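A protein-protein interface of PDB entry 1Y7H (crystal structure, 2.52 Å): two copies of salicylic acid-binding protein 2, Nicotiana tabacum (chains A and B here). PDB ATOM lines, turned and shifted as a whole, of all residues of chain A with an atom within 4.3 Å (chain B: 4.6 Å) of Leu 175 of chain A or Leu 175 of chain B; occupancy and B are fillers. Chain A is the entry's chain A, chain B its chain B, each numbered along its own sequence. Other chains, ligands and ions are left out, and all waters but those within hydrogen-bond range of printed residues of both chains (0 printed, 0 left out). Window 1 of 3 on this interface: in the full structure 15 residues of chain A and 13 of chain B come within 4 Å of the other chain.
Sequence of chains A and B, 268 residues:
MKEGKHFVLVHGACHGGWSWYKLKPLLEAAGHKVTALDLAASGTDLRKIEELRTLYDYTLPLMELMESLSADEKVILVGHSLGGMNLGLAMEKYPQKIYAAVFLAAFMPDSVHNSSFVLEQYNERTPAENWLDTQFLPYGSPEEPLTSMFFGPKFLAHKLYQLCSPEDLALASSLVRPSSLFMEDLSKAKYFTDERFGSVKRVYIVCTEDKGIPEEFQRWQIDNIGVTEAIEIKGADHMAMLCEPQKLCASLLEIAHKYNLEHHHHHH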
ATOM      1  N   TRP A  18     -16.612   0.189 -13.997  1.00  0.00           N
ATOM      2  CA  TRP A  18     -15.161   0.093 -14.120  1.00  0.00           C
ATOM      3  C   TRP A  18     -14.632   0.803 -15.352  1.00  0.00           C
ATOM      4  O   TRP A  18     -13.460   1.178 -15.403  1.00  0.00           O
ATOM      5  CB  TRP A  18     -14.706  -1.372 -14.175  1.00  0.00           C
ATOM      6  CG  TRP A  18     -15.353  -2.131 -15.270  1.00  0.00           C
ATOM      7  CD1 TRP A  18     -16.525  -2.819 -15.198  1.00  0.00           C
ATOM      8  CD2 TRP A  18     -14.912  -2.221 -16.631  1.00  0.00           C
ATOM      9  NE1 TRP A  18     -16.844  -3.334 -16.428  1.00  0.00           N
ATOM     10  CE2 TRP A  18     -15.873  -2.984 -17.326  1.00  0.00           C
ATOM     11  CE3 TRP A  18     -13.796  -1.735 -17.329  1.00  0.00           C
ATOM     12  CZ2 TRP A  18     -15.760  -3.267 -18.693  1.00  0.00           C
ATOM     13  CZ3 TRP A  18     -13.682  -2.019 -18.691  1.00  0.00           C
ATOM     14  CH2 TRP A  18     -14.662  -2.779 -19.356  1.00  0.00           C
ATOM     15  N   THR A  44     -19.990  -5.849 -11.225  1.00  0.00           N
ATOM     16  CA  THR A  44     -20.077  -6.857 -10.161  1.00  0.00           C
ATOM     17  C   THR A  44     -21.472  -7.090  -9.560  1.00  0.00           C
ATOM     18  O   THR A  44     -21.594  -7.684  -8.487  1.00  0.00           O
ATOM     19  CB  THR A  44     -19.136  -6.531  -8.982  1.00  0.00           C
ATOM     20  OG1 THR A  44     -19.685  -5.455  -8.210  1.00  0.00           O
ATOM     21  CG2 THR A  44     -17.755  -6.147  -9.485  1.00  0.00           C
ATOM     22  N   LEU A 171      -8.812  -5.839 -20.810  1.00  0.00           N
ATOM     23  CA  LEU A 171      -9.667  -5.594 -19.652  1.00  0.00           C
ATOM     24  C   LEU A 171     -11.121  -5.922 -20.001  1.00  0.00           C
ATOM     25  O   LEU A 171     -11.745  -6.761 -19.356  1.00  0.00           O
ATOM     26  CB  LEU A 171      -9.536  -4.129 -19.193  1.00  0.00           C
ATOM     27  CG  LEU A 171     -10.431  -3.630 -18.042  1.00  0.00           C
ATOM     28  CD1 LEU A 171     -10.124  -4.393 -16.768  1.00  0.00           C
ATOM     29  CD2 LEU A 171     -10.214  -2.119 -17.822  1.00  0.00           C
ATOM     30  N   ALA A 172     -11.641  -5.288 -21.046  1.00  0.00           N
ATOM     31  CA  ALA A 172     -13.022  -5.510 -21.458  1.00  0.00           C
ATOM     32  C   ALA A 172     -13.375  -6.979 -21.717  1.00  0.00           C
ATOM     33  O   ALA A 172     -14.395  -7.470 -21.235  1.00  0.00           O
ATOM     34  CB  ALA A 172     -13.338  -4.663 -22.694  1.00  0.00           C
ATOM     35  N   SER A 173     -12.540  -7.672 -22.483  1.00  0.00           N
ATOM     36  CA  SER A 173     -12.776  -9.075 -22.805  1.00  0.00           C
ATOM     37  C   SER A 173     -13.055  -9.882 -21.558  1.00  0.00           C
ATOM     38  O   SER A 173     -13.799 -10.870 -21.591  1.00  0.00           O
ATOM     39  CB  SER A 173     -11.561  -9.667 -23.512  1.00  0.00           C
ATOM     40  OG  SER A 173     -11.351  -9.027 -24.751  1.00  0.00           O
ATOM     41  N   SER A 174     -12.459  -9.465 -20.449  1.00  0.00           N
ATOM     42  CA  SER A 174     -12.662 -10.194 -19.212  1.00  0.00           C
ATOM     43  C   SER A 174     -13.735  -9.595 -18.315  1.00  0.00           C
ATOM     44  O   SER A 174     -13.977 -10.125 -17.238  1.00  0.00           O
ATOM     45  CB  SER A 174     -11.357 -10.286 -18.438  1.00  0.00           C
ATOM     46  OG  SER A 174     -11.219  -9.169 -17.592  1.00  0.00           O
ATOM     47  N   LEU A 175     -14.394  -8.522 -18.750  1.00  0.00           N
ATOM     48  CA  LEU A 175     -15.435  -7.904 -17.921  1.00  0.00           C
ATOM     49  C   LEU A 175     -16.775  -7.759 -18.608  1.00  0.00           C
ATOM     50  O   LEU A 175     -17.822  -7.804 -17.958  1.00  0.00           O
ATOM     51  CB  LEU A 175     -14.996  -6.523 -17.435  1.00  0.00           C
ATOM     52  CG  LEU A 175     -14.159  -6.429 -16.153  1.00  0.00           C
ATOM     53  CD1 LEU A 175     -13.449  -5.089 -16.096  1.00  0.00           C
ATOM     54  CD2 LEU A 175     -15.057  -6.617 -14.952  1.00  0.00           C
ATOM     55  N   VAL A 176     -16.746  -7.582 -19.924  1.00  0.00           N
ATOM     56  CA  VAL A 176     -17.981  -7.408 -20.664  1.00  0.00           C
ATOM     57  C   VAL A 176     -19.006  -8.482 -20.314  1.00  0.00           C
ATOM     58  O   VAL A 176     -18.700  -9.673 -20.322  1.00  0.00           O
ATOM     59  CB  VAL A 176     -17.724  -7.411 -22.176  1.00  0.00           C
ATOM     60  CG1 VAL A 176     -16.901  -6.195 -22.555  1.00  0.00           C
ATOM     61  CG2 VAL A 176     -17.035  -8.677 -22.584  1.00  0.00           C
ATOM     62  N   ARG A 177     -20.220  -8.053 -19.981  1.00  0.00           N
ATOM     63  CA  ARG A 177     -21.296  -8.982 -19.634  1.00  0.00           C
ATOM     64  C   ARG A 177     -22.493  -8.739 -20.554  1.00  0.00           C
ATOM     65  O   ARG A 177     -22.591  -7.711 -21.200  1.00  0.00           O
ATOM     66  CB  ARG A 177     -21.726  -8.798 -18.170  1.00  0.00           C
ATOM     67  CG  ARG A 177     -20.586  -8.793 -17.160  1.00  0.00           C
ATOM     68  CD  ARG A 177     -21.122  -8.505 -15.764  1.00  0.00           C
ATOM     69  NE  ARG A 177     -22.273  -9.361 -15.486  1.00  0.00           N
ATOM     70  CZ  ARG A 177     -22.987  -9.355 -14.365  1.00  0.00           C
ATOM     71  NH1 ARG A 177     -22.688  -8.534 -13.363  1.00  0.00           N
ATOM     72  NH2 ARG A 177     -24.020 -10.176 -14.265  1.00  0.00           N
ATOM     73  N   TRP B  18      -9.545  -9.898 -14.620  1.00  0.00           N
ATOM     74  CA  TRP B  18      -9.236  -8.561 -15.119  1.00  0.00           C
ATOM     75  C   TRP B  18      -7.888  -8.133 -14.589  1.00  0.00           C
ATOM     76  O   TRP B  18      -7.113  -7.498 -15.285  1.00  0.00           O
ATOM     77  CB  TRP B  18     -10.301  -7.548 -14.690  1.00  0.00           C
ATOM     78  CG  TRP B  18     -10.666  -7.599 -13.255  1.00  0.00           C
ATOM     79  CD1 TRP B  18     -11.639  -8.375 -12.675  1.00  0.00           C
ATOM     80  CD2 TRP B  18     -10.077  -6.836 -12.195  1.00  0.00           C
ATOM     81  NE1 TRP B  18     -11.691  -8.133 -11.321  1.00  0.00           N
ATOM     82  CE2 TRP B  18     -10.747  -7.193 -10.999  1.00  0.00           C
ATOM     83  CE3 TRP B  18      -9.051  -5.876 -12.139  1.00  0.00           C
ATOM     84  CZ2 TRP B  18     -10.425  -6.632  -9.764  1.00  0.00           C
ATOM     85  CZ3 TRP B  18      -8.728  -5.313 -10.901  1.00  0.00           C
ATOM     86  CH2 TRP B  18      -9.418  -5.695  -9.731  1.00  0.00           C
ATOM     87  N   THR B  44     -16.468 -11.787 -12.851  1.00  0.00           N
ATOM     88  CA  THR B  44     -17.835 -11.770 -13.353  1.00  0.00           C
ATOM     89  C   THR B  44     -18.566 -13.072 -13.087  1.00  0.00           C
ATOM     90  O   THR B  44     -19.717 -13.246 -13.494  1.00  0.00           O
ATOM     91  CB  THR B  44     -17.863 -11.465 -14.856  1.00  0.00           C
ATOM     92  OG1 THR B  44     -17.062 -12.423 -15.556  1.00  0.00           O
ATOM     93  CG2 THR B  44     -17.317 -10.076 -15.109  1.00  0.00           C
ATOM     94  N   LEU B 171     -10.006   1.319 -10.476  1.00  0.00           N
ATOM     95  CA  LEU B 171     -10.510   0.143 -11.171  1.00  0.00           C
ATOM     96  C   LEU B 171     -10.790  -0.949 -10.147  1.00  0.00           C
ATOM     97  O   LEU B 171     -11.909  -1.449 -10.035  1.00  0.00           O
ATOM     98  CB  LEU B 171      -9.468  -0.345 -12.169  1.00  0.00           C
ATOM     99  CG  LEU B 171      -9.712  -1.666 -12.890  1.00  0.00           C
ATOM    100  CD1 LEU B 171     -11.024  -1.624 -13.683  1.00  0.00           C
ATOM    101  CD2 LEU B 171      -8.538  -1.924 -13.820  1.00  0.00           C
ATOM    102  N   ALA B 172      -9.760  -1.303  -9.388  1.00  0.00           N
ATOM    103  CA  ALA B 172      -9.895  -2.344  -8.384  1.00  0.00           C
ATOM    104  C   ALA B 172     -11.030  -2.029  -7.426  1.00  0.00           C
ATOM    105  O   ALA B 172     -11.874  -2.883  -7.145  1.00  0.00           O
ATOM    106  CB  ALA B 172      -8.597  -2.510  -7.622  1.00  0.00           C
ATOM    107  N   SER B 173     -11.063  -0.807  -6.916  1.00  0.00           N
ATOM    108  CA  SER B 173     -12.137  -0.456  -6.002  1.00  0.00           C
ATOM    109  C   SER B 173     -13.480  -0.845  -6.613  1.00  0.00           C
ATOM    110  O   SER B 173     -14.360  -1.376  -5.929  1.00  0.00           O
ATOM    111  CB  SER B 173     -12.140   1.046  -5.707  1.00  0.00           C
ATOM    112  OG  SER B 173     -10.944   1.442  -5.073  1.00  0.00           O
ATOM    113  N   SER B 174     -13.626  -0.609  -7.910  1.00  0.00           N
ATOM    114  CA  SER B 174     -14.882  -0.890  -8.579  1.00  0.00           C
ATOM    115  C   SER B 174     -15.161  -2.327  -8.962  1.00  0.00           C
ATOM    116  O   SER B 174     -16.249  -2.624  -9.448  1.00  0.00           O
ATOM    117  CB  SER B 174     -15.007  -0.031  -9.831  1.00  0.00           C
ATOM    118  OG  SER B 174     -16.239  -0.320 -10.475  1.00  0.00           O
ATOM    119  N   LEU B 175     -14.190  -3.210  -8.753  1.00  0.00           N
ATOM    120  CA  LEU B 175     -14.357  -4.608  -9.111  1.00  0.00           C
ATOM    121  C   LEU B 175     -14.145  -5.593  -7.962  1.00  0.00           C
ATOM    122  O   LEU B 175     -14.680  -6.699  -8.001  1.00  0.00           O
ATOM    123  CB  LEU B 175     -13.419  -4.968 -10.271  1.00  0.00           C
ATOM    124  CG  LEU B 175     -13.626  -4.199 -11.575  1.00  0.00           C
ATOM    125  CD1 LEU B 175     -12.625  -4.680 -12.613  1.00  0.00           C
ATOM    126  CD2 LEU B 175     -15.052  -4.402 -12.081  1.00  0.00           C
ATOM    127  N   VAL B 176     -13.390  -5.209  -6.936  1.00  0.00           N
ATOM    128  CA  VAL B 176     -13.149  -6.141  -5.837  1.00  0.00           C
ATOM    129  C   VAL B 176     -14.438  -6.671  -5.204  1.00  0.00           C
ATOM    130  O   VAL B 176     -15.364  -5.910  -4.906  1.00  0.00           O
ATOM    131  CB  VAL B 176     -12.220  -5.538  -4.715  1.00  0.00           C
ATOM    132  CG1 VAL B 176     -10.795  -5.379  -5.241  1.00  0.00           C
ATOM    133  CG2 VAL B 176     -12.758  -4.211  -4.214  1.00  0.00           C
ATOM    134  N   ARG B 177     -14.488  -7.990  -5.021  1.00  0.00           N
ATOM    135  CA  ARG B 177     -15.635  -8.654  -4.417  1.00  0.00           C
ATOM    136  C   ARG B 177     -15.211  -9.455  -3.197  1.00  0.00           C
ATOM    137  O   ARG B 177     -14.024  -9.689  -2.980  1.00  0.00           O
ATOM    138  CB  ARG B 177     -16.286  -9.598  -5.417  1.00  0.00           C
ATOM    139  CG  ARG B 177     -16.805  -8.908  -6.643  1.00  0.00           C
ATOM    140  CD  ARG B 177     -17.199  -9.955  -7.622  1.00  0.00           C
ATOM    141  NE  ARG B 177     -18.288 -10.750  -7.064  1.00  0.00           N
ATOM    142  CZ  ARG B 177     -18.701 -11.908  -7.558  1.00  0.00           C
ATOM    143  NH1 ARG B 177     -18.109 -12.422  -8.625  1.00  0.00           N
ATOM    144  NH2 ARG B 177     -19.719 -12.529  -6.991  1.00  0.00           N
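N of Trp 18 of chain B lies close to OG of Ser 174 of chain A (3.5 Å).
The backbone carbonyl oxygen (O) of Leu 171 of chain A lies within hydrogen-bond range of the side-chain hydroxyl (OG) of Ser 174 of chain A (3.0 Å).
Among the printed residues, merely in contact across the chains: Trp 18 of chain A with Leu 171 of chain B (3.7 Å), Trp 18 of chain A with Ser 174 of chain B (3.6 Å), Trp 18 of chain A with Leu 175 of chain B (3.7 Å), Thr 44 of chain A with Ser 174 of chain B (3.8 Å), Thr 44 of chain A with Leu 175 of chain B (3.5 Å), Leu 171 of chain A with Trp 18 of chain B (3.8 Å), Ser 174 of chain A with Thr 44 of chain B (3.96 Å), Leu 175 of chain A with Thr 44 of chain B (3.7 Å) and Leu 175 of chain A with Leu 175 of chain B (3.6 Å).
Ala 172 of chain A touches none of the printed residues of chain B.
Of the printed residues of chain B, Ser 174 of chain A touches Trp 18 and Thr 44.
Leu 175 of chain A touches two residues of chain B.
Val 176 of chain A touches none of the printed residues of chain B.
Of the printed residues of chain A, Trp 18 of chain B touches Leu 171 and Ser 174.
Printed residues of chain A within 4 Å of Leu 171 of chain B: Trp 18 (3.7 Å).
Leu 175 of chain B touches just these residues of chain A: Trp 18 (3.7 Å), Thr 44 (3.5 Å) and Leu 175 (3.6 Å).
The nearest residue of chain B that does not touch Leu 175 of chain A is Trp 18 of chain B (4.2 Å).
Of the 9 printed residues of chain B, 5 touch a printed residue of chain A.
Hydrophobic or aromatic side chains of chain B that line the printed part of chain A: Trp 18, Leu 171 and Leu 175.
Among the printed residues, 10 pairs touch across the chains.
Among the printed residues, no Asp or Glu carboxylate lies within 4 Å of a Lys or Arg side-chain nitrogen of the other chain.
Trp 18 of chain A touches Ser 174 of chain B, and with the chains exchanged Ser 174 of chain A touches Trp 18 of chain B.
Trp 18 of chain A touches Leu 175 of chain B, but with the chains exchanged Leu 175 of chain A does not touch Trp 18 of chain B (4.2 Å).
Thr 44 of chain A touches Ser 174 of chain B, and with the chains exchanged Ser 174 of chain A touches Thr 44 of chain B.
Leu 175 of chain B touches its own counterpart, Leu 175 of chain A.
9 positions are printed for both chains.
Of the 10 pairs that touch across the chains among the printed residues, 9 have their exchanged pair printed and touching as well.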
